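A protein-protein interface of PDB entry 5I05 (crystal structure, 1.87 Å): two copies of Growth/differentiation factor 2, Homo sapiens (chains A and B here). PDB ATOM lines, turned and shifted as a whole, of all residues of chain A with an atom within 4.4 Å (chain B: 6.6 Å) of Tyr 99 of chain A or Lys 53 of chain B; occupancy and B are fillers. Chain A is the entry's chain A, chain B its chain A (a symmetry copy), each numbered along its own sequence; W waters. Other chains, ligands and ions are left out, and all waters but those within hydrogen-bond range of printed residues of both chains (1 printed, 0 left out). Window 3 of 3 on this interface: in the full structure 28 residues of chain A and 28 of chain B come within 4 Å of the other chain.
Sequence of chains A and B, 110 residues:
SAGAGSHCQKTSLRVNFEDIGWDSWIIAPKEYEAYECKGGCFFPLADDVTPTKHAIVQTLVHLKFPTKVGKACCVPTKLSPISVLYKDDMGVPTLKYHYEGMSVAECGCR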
ATOM      1  N   TRP A  25     -15.180  12.306 -40.815  1.00  0.00           N
ATOM      2  CA  TRP A  25     -15.063  13.469 -39.942  1.00  0.00           C
ATOM      3  C   TRP A  25     -14.542  13.148 -38.546  1.00  0.00           C
ATOM      4  O   TRP A  25     -14.360  14.074 -37.750  1.00  0.00           O
ATOM      5  CB  TRP A  25     -16.416  14.186 -39.834  1.00  0.00           C
ATOM      6  CG  TRP A  25     -17.391  13.548 -38.907  1.00  0.00           C
ATOM      7  CD1 TRP A  25     -18.137  12.432 -39.139  1.00  0.00           C
ATOM      8  CD2 TRP A  25     -17.741  14.003 -37.598  1.00  0.00           C
ATOM      9  NE1 TRP A  25     -18.928  12.156 -38.048  1.00  0.00           N
ATOM     10  CE2 TRP A  25     -18.702  13.108 -37.089  1.00  0.00           C
ATOM     11  CE3 TRP A  25     -17.333  15.076 -36.803  1.00  0.00           C
ATOM     12  CZ2 TRP A  25     -19.257  13.257 -35.824  1.00  0.00           C
ATOM     13  CZ3 TRP A  25     -17.885  15.217 -35.550  1.00  0.00           C
ATOM     14  CH2 TRP A  25     -18.834  14.318 -35.074  1.00  0.00           C
ATOM     15  N   PRO A  81     -21.006  11.074 -22.450  1.00  0.00           N
ATOM     16  CA  PRO A  81     -20.190  11.580 -23.555  1.00  0.00           C
ATOM     17  C   PRO A  81     -18.949  10.724 -23.766  1.00  0.00           C
ATOM     18  O   PRO A  81     -18.555   9.912 -22.930  1.00  0.00           O
ATOM     19  CB  PRO A  81     -19.810  12.988 -23.092  1.00  0.00           C
ATOM     20  CG  PRO A  81     -19.779  12.875 -21.594  1.00  0.00           C
ATOM     21  CD  PRO A  81     -20.839  11.881 -21.223  1.00  0.00           C
ATOM     22  N   ILE A  82     -18.321  10.940 -24.914  1.00  0.00           N
ATOM     23  CA  ILE A  82     -16.956  10.505 -25.155  1.00  0.00           C
ATOM     24  C   ILE A  82     -16.208  11.676 -25.779  1.00  0.00           C
ATOM     25  O   ILE A  82     -16.802  12.651 -26.234  1.00  0.00           O
ATOM     26  CB  ILE A  82     -16.882   9.262 -26.070  1.00  0.00           C
ATOM     27  CG1 ILE A  82     -17.355   9.597 -27.494  1.00  0.00           C
ATOM     28  CG2 ILE A  82     -17.724   8.133 -25.484  1.00  0.00           C
ATOM     29  CD1 ILE A  82     -17.109   8.501 -28.494  1.00  0.00           C
ATOM     30  N   VAL A  84     -13.841  12.905 -28.889  1.00  0.00           N
ATOM     31  CA  VAL A  84     -13.489  12.554 -30.257  1.00  0.00           C
ATOM     32  C   VAL A  84     -12.518  13.601 -30.779  1.00  0.00           C
ATOM     33  O   VAL A  84     -12.522  14.753 -30.338  1.00  0.00           O
ATOM     34  CB  VAL A  84     -14.729  12.444 -31.175  1.00  0.00           C
ATOM     35  CG1 VAL A  84     -15.659  11.335 -30.669  1.00  0.00           C
ATOM     36  CG2 VAL A  84     -15.462  13.768 -31.244  1.00  0.00           C
ATOM     37  N   LYS A  96     -13.053  17.425 -29.464  1.00  0.00           N
ATOM     38  CA  LYS A  96     -14.345  17.633 -28.826  1.00  0.00           C
ATOM     39  C   LYS A  96     -14.333  16.793 -27.552  1.00  0.00           C
ATOM     40  O   LYS A  96     -14.390  15.555 -27.607  1.00  0.00           O
ATOM     41  CB  LYS A  96     -15.492  17.263 -29.767  1.00  0.00           C
ATOM     42  CG  LYS A  96     -16.885  17.464 -29.184  1.00  0.00           C
ATOM     43  CD  LYS A  96     -17.138  18.899 -28.759  1.00  0.00           C
ATOM     44  CE  LYS A  96     -18.529  19.060 -28.163  1.00  0.00           C
ATOM     45  NZ  LYS A  96     -18.508  19.866 -26.912  1.00  0.00           N
ATOM     46  N   TYR A  97     -14.222  17.469 -26.409  1.00  0.00           N
ATOM     47  CA  TYR A  97     -13.891  16.782 -25.168  1.00  0.00           C
ATOM     48  C   TYR A  97     -15.094  16.015 -24.619  1.00  0.00           C
ATOM     49  O   TYR A  97     -14.968  14.847 -24.237  1.00  0.00           O
ATOM     50  CB  TYR A  97     -13.354  17.785 -24.147  1.00  0.00           C
ATOM     51  CG  TYR A  97     -12.838  17.142 -22.881  1.00  0.00           C
ATOM     52  CD1 TYR A  97     -11.817  16.196 -22.923  1.00  0.00           C
ATOM     53  CD2 TYR A  97     -13.367  17.477 -21.647  1.00  0.00           C
ATOM     54  CE1 TYR A  97     -11.347  15.600 -21.767  1.00  0.00           C
ATOM     55  CE2 TYR A  97     -12.904  16.884 -20.482  1.00  0.00           C
ATOM     56  CZ  TYR A  97     -11.891  15.951 -20.549  1.00  0.00           C
ATOM     57  OH  TYR A  97     -11.435  15.353 -19.395  1.00  0.00           O
ATOM     58  N   HIS A  98     -16.266  16.649 -24.577  1.00  0.00           N
ATOM     59  CA  HIS A  98     -17.518  15.981 -24.197  1.00  0.00           C
ATOM     60  C   HIS A  98     -18.431  15.937 -25.422  1.00  0.00           C
ATOM     61  O   HIS A  98     -19.253  16.831 -25.636  1.00  0.00           O
ATOM     62  CB  HIS A  98     -18.231  16.689 -23.040  1.00  0.00           C
ATOM     63  CG  HIS A  98     -17.424  16.778 -21.781  1.00  0.00           C
ATOM     64  ND1 HIS A  98     -17.076  15.671 -21.040  1.00  0.00           N
ATOM     65  CD2 HIS A  98     -16.936  17.848 -21.108  1.00  0.00           C
ATOM     66  CE1 HIS A  98     -16.386  16.051 -19.978  1.00  0.00           C
ATOM     67  NE2 HIS A  98     -16.290  17.369 -19.995  1.00  0.00           N
ATOM     68  N   TYR A  99     -18.310  14.875 -26.208  1.00  0.00           N
ATOM     69  CA  TYR A  99     -19.222  14.651 -27.328  1.00  0.00           C
ATOM     70  C   TYR A  99     -20.417  13.863 -26.793  1.00  0.00           C
ATOM     71  O   TYR A  99     -20.328  12.654 -26.560  1.00  0.00           O
ATOM     72  CB  TYR A  99     -18.507  13.928 -28.460  1.00  0.00           C
ATOM     73  CG  TYR A  99     -19.220  14.026 -29.783  1.00  0.00           C
ATOM     74  CD1 TYR A  99     -19.564  15.262 -30.315  1.00  0.00           C
ATOM     75  CD2 TYR A  99     -19.543  12.890 -30.502  1.00  0.00           C
ATOM     76  CE1 TYR A  99     -20.219  15.359 -31.526  1.00  0.00           C
ATOM     77  CE2 TYR A  99     -20.196  12.974 -31.710  1.00  0.00           C
ATOM     78  CZ  TYR A  99     -20.534  14.213 -32.216  1.00  0.00           C
ATOM     79  OH  TYR A  99     -21.183  14.302 -33.424  1.00  0.00           O
ATOM     80  N   GLU A 100     -21.532  14.555 -26.574  1.00  0.00           N
ATOM     81  CA  GLU A 100     -22.579  14.047 -25.692  1.00  0.00           C
ATOM     82  C   GLU A 100     -23.451  12.996 -26.368  1.00  0.00           C
ATOM     83  O   GLU A 100     -23.644  12.993 -27.585  1.00  0.00           O
ATOM     84  CB  GLU A 100     -23.463  15.191 -25.200  1.00  0.00           C
ATOM     85  CG  GLU A 100     -22.705  16.298 -24.457  1.00  0.00           C
ATOM     86  CD  GLU A 100     -22.318  15.915 -23.029  1.00  0.00           C
ATOM     87  OE1 GLU A 100     -22.753  14.846 -22.548  1.00  0.00           O
ATOM     88  OE2 GLU A 100     -21.573  16.685 -22.383  1.00  0.00           O
ATOM     89  N   GLY A 101     -23.989  12.099 -25.547  1.00  0.00           N
ATOM     90  CA  GLY A 101     -24.996  11.163 -25.997  1.00  0.00           C
ATOM     91  C   GLY A 101     -24.476   9.953 -26.726  1.00  0.00           C
ATOM     92  O   GLY A 101     -25.249   9.300 -27.432  1.00  0.00           O
ATOM     93  N   MET A 102     -23.205   9.596 -26.537  1.00  0.00           N
ATOM     94  CA  MET A 102     -22.576   8.569 -27.358  1.00  0.00           C
ATOM     95  C   MET A 102     -22.573   7.175 -26.734  1.00  0.00           C
ATOM     96  O   MET A 102     -22.505   6.195 -27.484  1.00  0.00           O
ATOM     97  CB  MET A 102     -21.134   8.985 -27.693  1.00  0.00           C
ATOM     98  CG  MET A 102     -21.073  10.141 -28.684  1.00  0.00           C
ATOM     99  SD  MET A 102     -21.646   9.654 -30.326  1.00  0.00           S
ATOM    100  CE  MET A 102     -20.233   8.698 -30.895  1.00  0.00           C
ATOM    101  N   PRO B  51     -33.505  12.583 -32.318  1.00  0.00           N
ATOM    102  CA  PRO B  51     -32.752  11.371 -32.010  1.00  0.00           C
ATOM    103  C   PRO B  51     -31.476  11.704 -31.263  1.00  0.00           C
ATOM    104  O   PRO B  51     -30.790  12.686 -31.554  1.00  0.00           O
ATOM    105  CB  PRO B  51     -32.461  10.772 -33.388  1.00  0.00           C
ATOM    106  CG  PRO B  51     -32.373  11.943 -34.258  1.00  0.00           C
ATOM    107  CD  PRO B  51     -33.385  12.935 -33.743  1.00  0.00           C
ATOM    108  N   THR B  52     -31.178  10.879 -30.276  1.00  0.00           N
ATOM    109  CA  THR B  52     -29.897  10.950 -29.613  1.00  0.00           C
ATOM    110  C   THR B  52     -28.806  10.454 -30.555  1.00  0.00           C
ATOM    111  O   THR B  52     -29.067   9.734 -31.528  1.00  0.00           O
ATOM    112  CB  THR B  52     -29.910  10.087 -28.359  1.00  0.00           C
ATOM    113  OG1 THR B  52     -30.125   8.730 -28.751  1.00  0.00           O
ATOM    114  CG2 THR B  52     -31.017  10.540 -27.405  1.00  0.00           C
ATOM    115  N   LYS B  53     -27.566  10.838 -30.252  1.00  0.00           N
ATOM    116  CA  LYS B  53     -26.436  10.333 -31.024  1.00  0.00           C
ATOM    117  C   LYS B  53     -26.353   8.817 -30.938  1.00  0.00           C
ATOM    118  O   LYS B  53     -26.039   8.148 -31.930  1.00  0.00           O
ATOM    119  CB  LYS B  53     -25.127  10.964 -30.536  1.00  0.00           C
ATOM    120  CG  LYS B  53     -25.044  12.471 -30.744  1.00  0.00           C
ATOM    121  CD  LYS B  53     -23.612  12.980 -30.626  1.00  0.00           C
ATOM    122  CE  LYS B  53     -23.565  14.504 -30.540  1.00  0.00           C
ATOM    123  NZ  LYS B  53     -24.128  15.041 -29.265  1.00  0.00           N
ATOM    124  N   HIS B  54     -26.636   8.250 -29.765  1.00  0.00           N
ATOM    125  CA  HIS B  54     -26.570   6.797 -29.645  1.00  0.00           C
ATOM    126  C   HIS B  54     -27.590   6.113 -30.555  1.00  0.00           C
ATOM    127  O   HIS B  54     -27.285   5.092 -31.170  1.00  0.00           O
ATOM    128  CB  HIS B  54     -26.772   6.349 -28.200  1.00  0.00           C
ATOM    129  CG  HIS B  54     -26.404   4.917 -27.989  1.00  0.00           C
ATOM    130  ND1 HIS B  54     -27.250   3.880 -28.312  1.00  0.00           N
ATOM    131  CD2 HIS B  54     -25.248   4.346 -27.581  1.00  0.00           C
ATOM    132  CE1 HIS B  54     -26.643   2.732 -28.079  1.00  0.00           C
ATOM    133  NE2 HIS B  54     -25.431   2.987 -27.624  1.00  0.00           N
ATOM    134  N   ALA B  55     -28.804   6.653 -30.651  1.00  0.00           N
ATOM    135  CA  ALA B  55     -29.801   6.058 -31.543  1.00  0.00           C
ATOM    136  C   ALA B  55     -29.336   6.084 -32.996  1.00  0.00           C
ATOM    137  O   ALA B  55     -29.574   5.137 -33.760  1.00  0.00           O
ATOM    138  CB  ALA B  55     -31.131   6.788 -31.405  1.00  0.00           C
ATOM    139  N   ILE B  56     -28.692   7.173 -33.404  1.00  0.00           N
ATOM    140  CA  ILE B  56     -28.175   7.262 -34.765  1.00  0.00           C
ATOM    141  C   ILE B  56     -27.081   6.223 -34.976  1.00  0.00           C
ATOM    142  O   ILE B  56     -27.070   5.475 -35.969  1.00  0.00           O
ATOM    143  CB  ILE B  56     -27.670   8.698 -35.023  1.00  0.00           C
ATOM    144  CG1 ILE B  56     -28.865   9.660 -34.973  1.00  0.00           C
ATOM    145  CG2 ILE B  56     -26.954   8.785 -36.348  1.00  0.00           C
ATOM    146  CD1 ILE B  56     -28.489  11.110 -34.815  1.00  0.00           C
ATOM    147  N   VAL B  57     -26.140   6.160 -34.038  1.00  0.00           N
ATOM    148  CA  VAL B  57     -25.051   5.194 -34.145  1.00  0.00           C
ATOM    149  C   VAL B  57     -25.602   3.777 -34.215  1.00  0.00           C
ATOM    150  O   VAL B  57     -25.173   2.961 -35.035  1.00  0.00           O
ATOM    151  CB  VAL B  57     -24.077   5.354 -32.966  1.00  0.00           C
ATOM    152  CG1 VAL B  57     -23.056   4.232 -32.979  1.00  0.00           C
ATOM    153  CG2 VAL B  57     -23.389   6.709 -33.042  1.00  0.00           C
ATOM    154  N   GLN B  58     -26.538   3.451 -33.330  1.00  0.00           N
ATOM    155  CA  GLN B  58     -27.047   2.091 -33.302  1.00  0.00           C
ATOM    156  C   GLN B  58     -27.791   1.765 -34.590  1.00  0.00           C
ATOM    157  O   GLN B  58     -27.687   0.650 -35.101  1.00  0.00           O
ATOM    158  CB  GLN B  58     -27.939   1.888 -32.076  1.00  0.00           C
ATOM    159  CG  GLN B  58     -28.402   0.439 -31.932  1.00  0.00           C
ATOM    160  CD  GLN B  58     -28.921   0.114 -30.546  1.00  0.00           C
ATOM    161  OE1 GLN B  58     -28.546   0.748 -29.555  1.00  0.00           O
ATOM    162  NE2 GLN B  58     -29.804  -0.875 -30.470  1.00  0.00           N
HETATM  163  O   HOH W   1     -21.922  17.405 -27.994  1.00  0.00           O
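O of Ile 82 of chain A sits at hydrogen-bond distance from N of Tyr 99 of chain A (2.7 Å).
O of Glu 100 of chain A lies within hydrogen-bond range of NZ of Lys 53 of chain B, at 2.7 Å. The backbone carbonyl oxygen (O) of Gly 101 of chain A sits at hydrogen-bond distance from the backbone NH (N) of His 54 of chain B (2.9 Å).
Among the printed residues, merely in contact across the chains: Met 102 of chain A with His 54 of chain B, Tyr 99 of chain A with Lys 53 of chain B, Gly 101 of chain A with Lys 53 of chain B and Met 102 of chain A with Lys 53 of chain B.
Of chain B, only Lys 53 (3.5 Å) comes within 4 Å of Tyr 99 of chain A. Printed residues of chain B within 4 Å of Glu 100 of chain A: Lys 53. Of the printed residues of chain B, Gly 101 of chain A touches Lys 53 and His 54. Of the printed residues of chain B, Met 102 of chain A touches Lys 53 and His 54. Thr 52 of chain B touches none of the printed residues of chain A. Of the printed residues of chain A, His 54 of chain B touches Gly 101 (2.9 Å) and Met 102 (3.3 Å). Ile 56 of chain B touches none of the printed residues of chain A. The nearest printed residue of chain B that does not touch Tyr 99 of chain A is Val 57 of chain B (7.2 Å). The nearest printed residue of chain A that does not touch His 54 of chain B is Glu 100 of chain A (6.0 Å).
No position is printed for both chains.
Water W1 lies within hydrogen-bond range of the backbone NH of Glu 100 of chain A (3.2 Å) and the side-chain amino group of Lys 53 of chain B (3.5 Å).
Of the 11 printed residues of chain A, 4 touch a printed residue of chain B.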
